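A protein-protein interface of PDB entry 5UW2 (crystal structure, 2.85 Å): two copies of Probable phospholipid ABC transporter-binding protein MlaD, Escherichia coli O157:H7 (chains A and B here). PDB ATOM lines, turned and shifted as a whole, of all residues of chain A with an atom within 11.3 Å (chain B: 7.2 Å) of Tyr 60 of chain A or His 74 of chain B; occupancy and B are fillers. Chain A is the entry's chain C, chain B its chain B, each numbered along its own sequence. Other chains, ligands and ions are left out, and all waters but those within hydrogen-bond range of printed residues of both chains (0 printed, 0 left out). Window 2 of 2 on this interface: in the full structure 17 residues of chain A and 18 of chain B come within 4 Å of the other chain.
Among the printed residues, merely in contact across the chains: Asp 29 of chain A with Gly 43 of chain B (3.4 Å), Asn 30 of chain A with Gly 43 of chain B (3.4 Å), Leu 55 of chain A with Ile 42 of chain B (3.8 Å), Leu 55 of chain A with Val 47 of chain B (3.3 Å), Leu 55 of chain A with Tyr 72 of chain B (3.7 Å), Tyr 60 of chain A with Ile 42 of chain B (3.8 Å), Tyr 60 of chain A with Tyr 72 of chain B (3.6 Å), Tyr 60 of chain A with Ile 75 of chain B (3.7 Å) and Pro 62 of chain A with Gly 43 of chain B (3.2 Å).
The side-chain hydroxyl of Tyr 22 of chain B lies within hydrogen-bond range of the backbone carbonyl oxygen of Tyr 72 of chain B, 2.9 Å away. The backbone carbonyl oxygen of Gln 70 of chain B is in hydrogen-bond range of the side-chain amide nitrogen of Asn 73 of chain B, 2.6 Å away. The guanidinium group of Arg 71 of chain B sits at hydrogen-bond distance from the side-chain hydroxyl of Tyr 72 of chain B (3.2 Å). The backbone carbonyl oxygen (O) of Ile 75 of chain B is in hydrogen-bond range of the backbone NH (N) of Leu 110 of chain B (3.0 Å). N of Asp 29 of chain A sits at hydrogen-bond distance from OG of Ser 121 of chain A, at 3.3 Å. The side-chain hydroxyl of Ser 121 of chain A lies within hydrogen-bond range of the backbone NH of Asn 30 of chain A, at 2.6 Å.
Printed residues of chain B within 4 Å of Asp 29 of chain A: Gly 43. Of the printed residues of chain B, Ile 31 of chain A touches Gly 43 (3.0 Å). Asn 73 of chain B touches just one residue of chain A: Tyr 60. No residue of chain A comes within 4 Å of Val 98 of chain B. The nearest printed residue of chain A that does not touch Tyr 72 of chain B is Thr 54 of chain A (5.6 Å).
No position is printed for both chains.
Hydrophobic or aromatic side chains of chain B within 4 Å of the printed part of chain A: Ile 42, Val 47, Tyr 72, His 74 and Ile 75. Along chain B the printed residues that touch a printed residue of chain A span positions 42 to 75. Along chain A the printed residues that touch a printed residue of chain B span positions 29 to 62. Among the printed residues, no Asp or Glu carboxylate lies within 4 Å of a Lys or Arg side-chain nitrogen of the other chain.
The backbone carbonyl oxygen (O) of Gly 43 of chain B lies within hydrogen-bond range of the backbone NH (N) of Ile 31 of chain A (3.0 Å). The side-chain hydroxyl (OH) of Tyr 60 of chain A lies within hydrogen-bond range of the backbone NH (N) of Asn 73 of chain B (3.4 Å). The backbone NH of His 74 of chain B sits at hydrogen-bond distance from the side-chain hydroxyl of Tyr 60 of chain A, at 2.7 Å.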
ATOM      1  N   ALA A  26      -9.752 -11.702 -16.732  1.00  0.00           N
ATOM      2  CA  ALA A  26      -9.177 -12.717 -17.613  1.00  0.00           C
ATOM      3  C   ALA A  26      -7.843 -12.269 -18.201  1.00  0.00           C
ATOM      4  O   ALA A  26      -7.762 -11.226 -18.847  1.00  0.00           O
ATOM      5  CB  ALA A  26     -10.154 -13.054 -18.728  1.00  0.00           C
ATOM      6  N   THR A  27      -6.805 -13.073 -17.987  1.00  0.00           N
ATOM      7  CA  THR A  27      -5.470 -12.762 -18.492  1.00  0.00           C
ATOM      8  C   THR A  27      -5.186 -13.502 -19.798  1.00  0.00           C
ATOM      9  O   THR A  27      -5.449 -14.700 -19.917  1.00  0.00           O
ATOM     10  CB  THR A  27      -4.381 -13.122 -17.459  1.00  0.00           C
ATOM     11  OG1 THR A  27      -4.655 -12.456 -16.221  1.00  0.00           O
ATOM     12  CG2 THR A  27      -3.000 -12.711 -17.960  1.00  0.00           C
ATOM     13  N   PHE A  28      -4.648 -12.769 -20.770  1.00  0.00           N
ATOM     14  CA  PHE A  28      -4.284 -13.316 -22.074  1.00  0.00           C
ATOM     15  C   PHE A  28      -2.791 -13.145 -22.326  1.00  0.00           C
ATOM     16  O   PHE A  28      -2.104 -12.459 -21.570  1.00  0.00           O
ATOM     17  CB  PHE A  28      -5.073 -12.625 -23.191  1.00  0.00           C
ATOM     18  CG  PHE A  28      -6.557 -12.837 -23.116  1.00  0.00           C
ATOM     19  CD1 PHE A  28      -7.327 -12.140 -22.200  1.00  0.00           C
ATOM     20  CD2 PHE A  28      -7.187 -13.718 -23.979  1.00  0.00           C
ATOM     21  CE1 PHE A  28      -8.694 -12.331 -22.134  1.00  0.00           C
ATOM     22  CE2 PHE A  28      -8.553 -13.912 -23.920  1.00  0.00           C
ATOM     23  CZ  PHE A  28      -9.308 -13.218 -22.997  1.00  0.00           C
ATOM     24  N   ASP A  29      -2.294 -13.785 -23.380  1.00  0.00           N
ATOM     25  CA  ASP A  29      -0.935 -13.548 -23.856  1.00  0.00           C
ATOM     26  C   ASP A  29      -0.955 -12.399 -24.858  1.00  0.00           C
ATOM     27  O   ASP A  29       0.003 -11.633 -24.967  1.00  0.00           O
ATOM     28  CB  ASP A  29      -0.346 -14.808 -24.497  1.00  0.00           C
ATOM     29  CG  ASP A  29      -0.022 -15.889 -23.480  1.00  0.00           C
ATOM     30  OD1 ASP A  29       0.342 -15.546 -22.335  1.00  0.00           O
ATOM     31  OD2 ASP A  29      -0.123 -17.084 -23.831  1.00  0.00           O
ATOM     32  N   ASN A  30      -2.060 -12.299 -25.590  1.00  0.00           N
ATOM     33  CA  ASN A  30      -2.260 -11.240 -26.572  1.00  0.00           C
ATOM     34  C   ASN A  30      -3.746 -10.938 -26.735  1.00  0.00           C
ATOM     35  O   ASN A  30      -4.539 -11.838 -27.016  1.00  0.00           O
ATOM     36  CB  ASN A  30      -1.649 -11.633 -27.920  1.00  0.00           C
ATOM     37  CG  ASN A  30      -1.632 -10.485 -28.920  1.00  0.00           C
ATOM     38  OD1 ASN A  30      -2.615  -9.760 -29.077  1.00  0.00           O
ATOM     39  ND2 ASN A  30      -0.506 -10.316 -29.602  1.00  0.00           N
ATOM     40  N   ILE A  31      -4.117  -9.672 -26.562  1.00  0.00           N
ATOM     41  CA  ILE A  31      -5.514  -9.266 -26.684  1.00  0.00           C
ATOM     42  C   ILE A  31      -5.831  -8.776 -28.096  1.00  0.00           C
ATOM     43  O   ILE A  31      -6.997  -8.662 -28.476  1.00  0.00           O
ATOM     44  CB  ILE A  31      -5.878  -8.162 -25.679  1.00  0.00           C
ATOM     45  CG1 ILE A  31      -4.966  -6.944 -25.853  1.00  0.00           C
ATOM     46  CG2 ILE A  31      -5.802  -8.703 -24.258  1.00  0.00           C
ATOM     47  CD1 ILE A  31      -5.683  -5.634 -25.668  1.00  0.00           C
ATOM     48  N   ILE A  53      -8.509  -2.736 -19.615  1.00  0.00           N
ATOM     49  CA  ILE A  53      -7.401  -3.591 -20.030  1.00  0.00           C
ATOM     50  C   ILE A  53      -6.097  -3.024 -19.482  1.00  0.00           C
ATOM     51  O   ILE A  53      -5.800  -1.845 -19.677  1.00  0.00           O
ATOM     52  CB  ILE A  53      -7.306  -3.709 -21.564  1.00  0.00           C
ATOM     53  CG1 ILE A  53      -8.608  -4.288 -22.132  1.00  0.00           C
ATOM     54  CG2 ILE A  53      -6.116  -4.578 -21.955  1.00  0.00           C
ATOM     55  CD1 ILE A  53      -8.681  -4.291 -23.647  1.00  0.00           C
ATOM     56  N   THR A  54      -5.323  -3.859 -18.794  1.00  0.00           N
ATOM     57  CA  THR A  54      -4.065  -3.404 -18.205  1.00  0.00           C
ATOM     58  C   THR A  54      -3.048  -4.532 -18.076  1.00  0.00           C
ATOM     59  O   THR A  54      -3.380  -5.634 -17.653  1.00  0.00           O
ATOM     60  CB  THR A  54      -4.299  -2.778 -16.813  1.00  0.00           C
ATOM     61  OG1 THR A  54      -5.149  -1.630 -16.935  1.00  0.00           O
ATOM     62  CG2 THR A  54      -2.980  -2.356 -16.169  1.00  0.00           C
ATOM     63  N   LEU A  55      -1.804  -4.239 -18.440  1.00  0.00           N
ATOM     64  CA  LEU A  55      -0.709  -5.193 -18.289  1.00  0.00           C
ATOM     65  C   LEU A  55      -0.382  -5.404 -16.814  1.00  0.00           C
ATOM     66  O   LEU A  55      -0.163  -4.443 -16.075  1.00  0.00           O
ATOM     67  CB  LEU A  55       0.535  -4.706 -19.034  1.00  0.00           C
ATOM     68  CG  LEU A  55       0.504  -4.805 -20.560  1.00  0.00           C
ATOM     69  CD1 LEU A  55       1.659  -4.030 -21.170  1.00  0.00           C
ATOM     70  CD2 LEU A  55       0.554  -6.257 -20.998  1.00  0.00           C
ATOM     71  N   ASP A  56      -0.359  -6.664 -16.390  1.00  0.00           N
ATOM     72  CA  ASP A  56       0.011  -7.003 -15.020  1.00  0.00           C
ATOM     73  C   ASP A  56       1.429  -6.525 -14.712  1.00  0.00           C
ATOM     74  O   ASP A  56       2.343  -6.758 -15.503  1.00  0.00           O
ATOM     75  CB  ASP A  56      -0.093  -8.512 -14.795  1.00  0.00           C
ATOM     76  CG  ASP A  56       0.433  -8.936 -13.437  1.00  0.00           C
ATOM     77  OD1 ASP A  56      -0.338  -8.914 -12.455  1.00  0.00           O
ATOM     78  OD2 ASP A  56       1.626  -9.292 -13.350  1.00  0.00           O
ATOM     79  N   PRO A  57       1.615  -5.848 -13.565  1.00  0.00           N
ATOM     80  CA  PRO A  57       2.923  -5.251 -13.269  1.00  0.00           C
ATOM     81  C   PRO A  57       4.037  -6.285 -13.139  1.00  0.00           C
ATOM     82  O   PRO A  57       5.192  -5.981 -13.435  1.00  0.00           O
ATOM     83  CB  PRO A  57       2.687  -4.538 -11.932  1.00  0.00           C
ATOM     84  CG  PRO A  57       1.549  -5.261 -11.311  1.00  0.00           C
ATOM     85  CD  PRO A  57       0.667  -5.663 -12.451  1.00  0.00           C
ATOM     86  N   LYS A  58       3.686  -7.492 -12.708  1.00  0.00           N
ATOM     87  CA  LYS A  58       4.676  -8.534 -12.461  1.00  0.00           C
ATOM     88  C   LYS A  58       4.994  -9.343 -13.718  1.00  0.00           C
ATOM     89  O   LYS A  58       6.160  -9.606 -14.014  1.00  0.00           O
ATOM     90  CB  LYS A  58       4.179  -9.478 -11.361  1.00  0.00           C
ATOM     91  CG  LYS A  58       3.926  -8.807 -10.019  1.00  0.00           C
ATOM     92  CD  LYS A  58       3.556  -9.830  -8.955  1.00  0.00           C
ATOM     93  CE  LYS A  58       3.234  -9.172  -7.624  1.00  0.00           C
ATOM     94  NZ  LYS A  58       4.429  -8.531  -7.010  1.00  0.00           N
ATOM     95  N   THR A  59       3.954  -9.729 -14.453  1.00  0.00           N
ATOM     96  CA  THR A  59       4.093 -10.677 -15.558  1.00  0.00           C
ATOM     97  C   THR A  59       4.121 -10.035 -16.946  1.00  0.00           C
ATOM     98  O   THR A  59       4.438 -10.707 -17.928  1.00  0.00           O
ATOM     99  CB  THR A  59       2.947 -11.708 -15.541  1.00  0.00           C
ATOM    100  OG1 THR A  59       1.701 -11.050 -15.799  1.00  0.00           O
ATOM    101  CG2 THR A  59       2.878 -12.414 -14.196  1.00  0.00           C
ATOM    102  N   TYR A  60       3.788  -8.749 -17.027  1.00  0.00           N
ATOM    103  CA  TYR A  60       3.726  -8.045 -18.310  1.00  0.00           C
ATOM    104  C   TYR A  60       2.755  -8.733 -19.276  1.00  0.00           C
ATOM    105  O   TYR A  60       2.926  -8.671 -20.495  1.00  0.00           O
ATOM    106  CB  TYR A  60       5.123  -7.942 -18.941  1.00  0.00           C
ATOM    107  CG  TYR A  60       5.949  -6.790 -18.421  1.00  0.00           C
ATOM    108  CD1 TYR A  60       6.426  -6.781 -17.118  1.00  0.00           C
ATOM    109  CD2 TYR A  60       6.263  -5.715 -19.242  1.00  0.00           C
ATOM    110  CE1 TYR A  60       7.185  -5.728 -16.643  1.00  0.00           C
ATOM    111  CE2 TYR A  60       7.021  -4.660 -18.779  1.00  0.00           C
ATOM    112  CZ  TYR A  60       7.480  -4.670 -17.479  1.00  0.00           C
ATOM    113  OH  TYR A  60       8.236  -3.618 -17.014  1.00  0.00           O
ATOM    114  N   LEU A  61       1.737  -9.383 -18.719  1.00  0.00           N
ATOM    115  CA  LEU A  61       0.701 -10.031 -19.521  1.00  0.00           C
ATOM    116  C   LEU A  61      -0.598  -9.224 -19.463  1.00  0.00           C
ATOM    117  O   LEU A  61      -0.979  -8.743 -18.395  1.00  0.00           O
ATOM    118  CB  LEU A  61       0.453 -11.462 -19.036  1.00  0.00           C
ATOM    119  CG  LEU A  61       1.603 -12.464 -19.184  1.00  0.00           C
ATOM    120  CD1 LEU A  61       1.153 -13.848 -18.746  1.00  0.00           C
ATOM    121  CD2 LEU A  61       2.135 -12.507 -20.612  1.00  0.00           C
ATOM    122  N   PRO A  62      -1.280  -9.068 -20.612  1.00  0.00           N
ATOM    123  CA  PRO A  62      -2.546  -8.324 -20.629  1.00  0.00           C
ATOM    124  C   PRO A  62      -3.617  -8.904 -19.708  1.00  0.00           C
ATOM    125  O   PRO A  62      -4.030 -10.052 -19.884  1.00  0.00           O
ATOM    126  CB  PRO A  62      -2.991  -8.424 -22.091  1.00  0.00           C
ATOM    127  CG  PRO A  62      -1.747  -8.625 -22.855  1.00  0.00           C
ATOM    128  CD  PRO A  62      -0.840  -9.423 -21.974  1.00  0.00           C
ATOM    129  N   ARG A  63      -4.049  -8.106 -18.736  1.00  0.00           N
ATOM    130  CA  ARG A  63      -5.180  -8.456 -17.886  1.00  0.00           C
ATOM    131  C   ARG A  63      -6.418  -7.692 -18.338  1.00  0.00           C
ATOM    132  O   ARG A  63      -6.425  -6.456 -18.366  1.00  0.00           O
ATOM    133  CB  ARG A  63      -4.888  -8.151 -16.414  1.00  0.00           C
ATOM    134  CG  ARG A  63      -6.072  -8.411 -15.490  1.00  0.00           C
ATOM    135  CD  ARG A  63      -5.728  -8.147 -14.033  1.00  0.00           C
ATOM    136  NE  ARG A  63      -4.776  -9.120 -13.497  1.00  0.00           N
ATOM    137  CZ  ARG A  63      -3.513  -8.855 -13.165  1.00  0.00           C
ATOM    138  NH1 ARG A  63      -3.005  -7.635 -13.310  1.00  0.00           N
ATOM    139  NH2 ARG A  63      -2.749  -9.824 -12.684  1.00  0.00           N
ATOM    140  N   VAL A  64      -7.454  -8.442 -18.699  1.00  0.00           N
ATOM    141  CA  VAL A  64      -8.719  -7.869 -19.135  1.00  0.00           C
ATOM    142  C   VAL A  64      -9.726  -7.895 -17.991  1.00  0.00           C
ATOM    143  O   VAL A  64     -10.013  -8.955 -17.421  1.00  0.00           O
ATOM    144  CB  VAL A  64      -9.300  -8.630 -20.347  1.00  0.00           C
ATOM    145  CG1 VAL A  64     -10.600  -7.989 -20.811  1.00  0.00           C
ATOM    146  CG2 VAL A  64      -8.294  -8.668 -21.486  1.00  0.00           C
ATOM    147  N   SER A 121      -6.081 -16.607 -26.926  1.00  0.00           N
ATOM    148  CA  SER A 121      -5.565 -15.308 -27.339  1.00  0.00           C
ATOM    149  C   SER A 121      -6.016 -14.932 -28.748  1.00  0.00           C
ATOM    150  O   SER A 121      -6.669 -15.717 -29.436  1.00  0.00           O
ATOM    151  CB  SER A 121      -4.037 -15.301 -27.270  1.00  0.00           C
ATOM    152  OG  SER A 121      -3.577 -14.258 -26.433  1.00  0.00           O
ATOM    153  N   TYR B  22      11.113   6.626 -21.904  1.00  0.00           N
ATOM    154  CA  TYR B  22      12.538   6.428 -22.142  1.00  0.00           C
ATOM    155  C   TYR B  22      12.762   5.944 -23.572  1.00  0.00           C
ATOM    156  O   TYR B  22      11.913   5.258 -24.153  1.00  0.00           O
ATOM    157  CB  TYR B  22      13.132   5.442 -21.131  1.00  0.00           C
ATOM    158  CG  TYR B  22      12.602   4.030 -21.220  1.00  0.00           C
ATOM    159  CD1 TYR B  22      11.391   3.682 -20.636  1.00  0.00           C
ATOM    160  CD2 TYR B  22      13.325   3.038 -21.868  1.00  0.00           C
ATOM    161  CE1 TYR B  22      10.909   2.388 -20.709  1.00  0.00           C
ATOM    162  CE2 TYR B  22      12.852   1.744 -21.945  1.00  0.00           C
ATOM    163  CZ  TYR B  22      11.643   1.424 -21.365  1.00  0.00           C
ATOM    164  OH  TYR B  22      11.167   0.135 -21.439  1.00  0.00           O
ATOM    165  N   ILE B  42       2.810  -4.289 -26.221  1.00  0.00           N
ATOM    166  CA  ILE B  42       3.120  -5.571 -25.601  1.00  0.00           C
ATOM    167  C   ILE B  42       1.819  -6.340 -25.411  1.00  0.00           C
ATOM    168  O   ILE B  42       0.888  -5.849 -24.770  1.00  0.00           O
ATOM    169  CB  ILE B  42       3.831  -5.398 -24.239  1.00  0.00           C
ATOM    170  CG1 ILE B  42       5.166  -4.676 -24.425  1.00  0.00           C
ATOM    171  CG2 ILE B  42       4.054  -6.753 -23.570  1.00  0.00           C
ATOM    172  CD1 ILE B  42       5.821  -4.239 -23.122  1.00  0.00           C
ATOM    173  N   GLY B  43       1.756  -7.540 -25.981  1.00  0.00           N
ATOM    174  CA  GLY B  43       0.564  -8.367 -25.902  1.00  0.00           C
ATOM    175  C   GLY B  43      -0.670  -7.654 -26.425  1.00  0.00           C
ATOM    176  O   GLY B  43      -1.788  -7.921 -25.978  1.00  0.00           O
ATOM    177  N   VAL B  47       2.181   0.290 -25.225  1.00  0.00           N
ATOM    178  CA  VAL B  47       3.037   0.709 -24.118  1.00  0.00           C
ATOM    179  C   VAL B  47       4.008   1.808 -24.543  1.00  0.00           C
ATOM    180  O   VAL B  47       4.756   2.333 -23.719  1.00  0.00           O
ATOM    181  CB  VAL B  47       3.851  -0.475 -23.555  1.00  0.00           C
ATOM    182  CG1 VAL B  47       2.922  -1.528 -22.965  1.00  0.00           C
ATOM    183  CG2 VAL B  47       4.742  -1.081 -24.636  1.00  0.00           C
ATOM    184  N   GLN B  70       7.446   5.290 -19.149  1.00  0.00           N
ATOM    185  CA  GLN B  70       8.387   5.135 -18.051  1.00  0.00           C
ATOM    186  C   GLN B  70       7.962   4.040 -17.078  1.00  0.00           C
ATOM    187  O   GLN B  70       8.804   3.444 -16.416  1.00  0.00           O
ATOM    188  CB  GLN B  70       8.537   6.468 -17.308  1.00  0.00           C
ATOM    189  CG  GLN B  70       9.570   6.492 -16.183  1.00  0.00           C
ATOM    190  CD  GLN B  70      10.979   6.190 -16.654  1.00  0.00           C
ATOM    191  OE1 GLN B  70      11.443   6.737 -17.655  1.00  0.00           O
ATOM    192  NE2 GLN B  70      11.685   5.347 -15.910  1.00  0.00           N
ATOM    193  N   ARG B  71       6.662   3.774 -16.985  1.00  0.00           N
ATOM    194  CA  ARG B  71       6.173   2.821 -15.992  1.00  0.00           C
ATOM    195  C   ARG B  71       6.433   1.368 -16.401  1.00  0.00           C
ATOM    196  O   ARG B  71       6.272   0.458 -15.588  1.00  0.00           O
ATOM    197  CB  ARG B  71       4.678   3.036 -15.727  1.00  0.00           C
ATOM    198  CG  ARG B  71       3.736   2.742 -16.890  1.00  0.00           C
ATOM    199  CD  ARG B  71       2.289   2.940 -16.445  1.00  0.00           C
ATOM    200  NE  ARG B  71       1.308   2.475 -17.425  1.00  0.00           N
ATOM    201  CZ  ARG B  71       0.694   3.247 -18.319  1.00  0.00           C
ATOM    202  NH1 ARG B  71       0.945   4.550 -18.382  1.00  0.00           N
ATOM    203  NH2 ARG B  71      -0.181   2.713 -19.158  1.00  0.00           N
ATOM    204  N   TYR B  72       6.832   1.154 -17.653  1.00  0.00           N
ATOM    205  CA  TYR B  72       7.251  -0.170 -18.114  1.00  0.00           C
ATOM    206  C   TYR B  72       8.776  -0.272 -18.181  1.00  0.00           C
ATOM    207  O   TYR B  72       9.358  -0.254 -19.266  1.00  0.00           O
ATOM    208  CB  TYR B  72       6.638  -0.481 -19.482  1.00  0.00           C
ATOM    209  CG  TYR B  72       5.127  -0.427 -19.498  1.00  0.00           C
ATOM    210  CD1 TYR B  72       4.371  -1.418 -18.886  1.00  0.00           C
ATOM    211  CD2 TYR B  72       4.455   0.611 -20.129  1.00  0.00           C
ATOM    212  CE1 TYR B  72       2.990  -1.374 -18.897  1.00  0.00           C
ATOM    213  CE2 TYR B  72       3.075   0.662 -20.146  1.00  0.00           C
ATOM    214  CZ  TYR B  72       2.348  -0.332 -19.529  1.00  0.00           C
ATOM    215  OH  TYR B  72       0.973  -0.284 -19.545  1.00  0.00           O
ATOM    216  N   ASN B  73       9.412  -0.382 -17.017  1.00  0.00           N
ATOM    217  CA  ASN B  73      10.872  -0.364 -16.928  1.00  0.00           C
ATOM    218  C   ASN B  73      11.503  -1.743 -17.017  1.00  0.00           C
ATOM    219  O   ASN B  73      12.604  -1.895 -17.542  1.00  0.00           O
ATOM    220  CB  ASN B  73      11.326   0.285 -15.619  1.00  0.00           C
ATOM    221  CG  ASN B  73      10.901   1.722 -15.509  1.00  0.00           C
ATOM    222  OD1 ASN B  73      10.308   2.132 -14.511  1.00  0.00           O
ATOM    223  ND2 ASN B  73      11.187   2.503 -16.545  1.00  0.00           N
ATOM    224  N   HIS B  74      10.795  -2.747 -16.515  1.00  0.00           N
ATOM    225  CA  HIS B  74      11.397  -4.050 -16.270  1.00  0.00           C
ATOM    226  C   HIS B  74      11.397  -4.929 -17.518  1.00  0.00           C
ATOM    227  O   HIS B  74      11.138  -6.130 -17.441  1.00  0.00           O
ATOM    228  CB  HIS B  74      10.655  -4.749 -15.129  1.00  0.00           C
ATOM    229  CG  HIS B  74      11.489  -5.742 -14.384  1.00  0.00           C
ATOM    230  ND1 HIS B  74      12.513  -5.367 -13.542  1.00  0.00           N
ATOM    231  CD2 HIS B  74      11.450  -7.095 -14.349  1.00  0.00           C
ATOM    232  CE1 HIS B  74      13.071  -6.445 -13.022  1.00  0.00           C
ATOM    233  NE2 HIS B  74      12.444  -7.507 -13.496  1.00  0.00           N
ATOM    234  N   ILE B  75      11.695  -4.320 -18.663  1.00  0.00           N
ATOM    235  CA  ILE B  75      11.792  -5.045 -19.925  1.00  0.00           C
ATOM    236  C   ILE B  75      13.241  -5.485 -20.145  1.00  0.00           C
ATOM    237  O   ILE B  75      14.122  -4.639 -20.296  1.00  0.00           O
ATOM    238  CB  ILE B  75      11.322  -4.181 -21.113  1.00  0.00           C
ATOM    239  CG1 ILE B  75       9.897  -3.674 -20.860  1.00  0.00           C
ATOM    240  CG2 ILE B  75      11.406  -4.977 -22.418  1.00  0.00           C
ATOM    241  CD1 ILE B  75       9.351  -2.758 -21.939  1.00  0.00           C
ATOM    242  N   PRO B  76      13.497  -6.807 -20.165  1.00  0.00           N
ATOM    243  CA  PRO B  76      14.878  -7.266 -20.370  1.00  0.00           C
ATOM    244  C   PRO B  76      15.419  -6.937 -21.758  1.00  0.00           C
ATOM    245  O   PRO B  76      14.646  -6.622 -22.664  1.00  0.00           O
ATOM    246  CB  PRO B  76      14.781  -8.787 -20.175  1.00  0.00           C
ATOM    247  CG  PRO B  76      13.499  -9.014 -19.457  1.00  0.00           C
ATOM    248  CD  PRO B  76      12.582  -7.933 -19.914  1.00  0.00           C
ATOM    249  N   SER B  79      14.471  -9.076 -24.994  1.00  0.00           N
ATOM    250  CA  SER B  79      13.171  -8.882 -25.628  1.00  0.00           C
ATOM    251  C   SER B  79      13.303  -8.662 -27.133  1.00  0.00           C
ATOM    252  O   SER B  79      14.343  -8.207 -27.612  1.00  0.00           O
ATOM    253  CB  SER B  79      12.450  -7.699 -24.985  1.00  0.00           C
ATOM    254  OG  SER B  79      12.271  -7.915 -23.595  1.00  0.00           O
ATOM    255  N   LEU B  96       6.387  -5.720 -29.228  1.00  0.00           N
ATOM    256  CA  LEU B  96       7.534  -5.953 -28.357  1.00  0.00           C
ATOM    257  C   LEU B  96       7.327  -7.211 -27.517  1.00  0.00           C
ATOM    258  O   LEU B  96       6.556  -7.200 -26.556  1.00  0.00           O
ATOM    259  CB  LEU B  96       7.766  -4.742 -27.449  1.00  0.00           C
ATOM    260  CG  LEU B  96       8.952  -4.814 -26.483  1.00  0.00           C
ATOM    261  CD1 LEU B  96      10.273  -4.827 -27.233  1.00  0.00           C
ATOM    262  CD2 LEU B  96       8.911  -3.651 -25.510  1.00  0.00           C
ATOM    263  N   VAL B  98       8.349  -9.544 -24.734  1.00  0.00           N
ATOM    264  CA  VAL B  98       9.169  -9.532 -23.527  1.00  0.00           C
ATOM    265  C   VAL B  98       9.911 -10.856 -23.361  1.00  0.00           C
ATOM    266  O   VAL B  98       9.290 -11.916 -23.282  1.00  0.00           O
ATOM    267  CB  VAL B  98       8.316  -9.266 -22.267  1.00  0.00           C
ATOM    268  CG1 VAL B  98       9.191  -9.208 -21.021  1.00  0.00           C
ATOM    269  CG2 VAL B  98       7.524  -7.977 -22.421  1.00  0.00           C
ATOM    270  N   GLY B  99      11.239 -10.791 -23.307  1.00  0.00           N
ATOM    271  CA  GLY B  99      12.048 -11.983 -23.124  1.00  0.00           C
ATOM    272  C   GLY B  99      12.101 -12.410 -21.669  1.00  0.00           C
ATOM    273  O   GLY B  99      11.725 -11.644 -20.782  1.00  0.00           O
ATOM    274  N   GLU B 101      14.202 -13.685 -18.170  1.00  0.00           N
ATOM    275  CA  GLU B 101      15.419 -13.244 -17.496  1.00  0.00           C
ATOM    276  C   GLU B 101      15.994 -14.364 -16.636  1.00  0.00           C
ATOM    277  O   GLU B 101      15.273 -15.266 -16.212  1.00  0.00           O
ATOM    278  CB  GLU B 101      15.144 -12.009 -16.637  1.00  0.00           C
ATOM    279  CG  GLU B 101      16.381 -11.454 -15.946  1.00  0.00           C
ATOM    280  CD  GLU B 101      16.095 -10.189 -15.162  1.00  0.00           C
ATOM    281  OE1 GLU B 101      14.932  -9.732 -15.169  1.00  0.00           O
ATOM    282  OE2 GLU B 101      17.035  -9.652 -14.538  1.00  0.00           O
ATOM    283  N   ILE B 109      18.345  -5.194 -17.592  1.00  0.00           N
ATOM    284  CA  ILE B 109      17.176  -4.399 -17.956  1.00  0.00           C
ATOM    285  C   ILE B 109      17.521  -3.318 -18.981  1.00  0.00           C
ATOM    286  O   ILE B 109      18.620  -2.763 -18.968  1.00  0.00           O
ATOM    287  CB  ILE B 109      16.549  -3.736 -16.707  1.00  0.00           C
ATOM    288  CG1 ILE B 109      16.166  -4.791 -15.664  1.00  0.00           C
ATOM    289  CG2 ILE B 109      15.339  -2.888 -17.083  1.00  0.00           C
ATOM    290  CD1 ILE B 109      15.134  -5.804 -16.136  1.00  0.00           C
ATOM    291  N   LEU B 110      16.572  -3.031 -19.869  1.00  0.00           N
ATOM    292  CA  LEU B 110      16.736  -1.987 -20.879  1.00  0.00           C
ATOM    293  C   LEU B 110      16.520  -0.596 -20.285  1.00  0.00           C
ATOM    294  O   LEU B 110      15.520  -0.353 -19.608  1.00  0.00           O
ATOM    295  CB  LEU B 110      15.763  -2.210 -22.038  1.00  0.00           C
ATOM    296  CG  LEU B 110      16.032  -3.421 -22.935  1.00  0.00           C
ATOM    297  CD1 LEU B 110      14.871  -3.637 -23.892  1.00  0.00           C
ATOM    298  CD2 LEU B 110      17.335  -3.243 -23.706  1.00  0.00           C
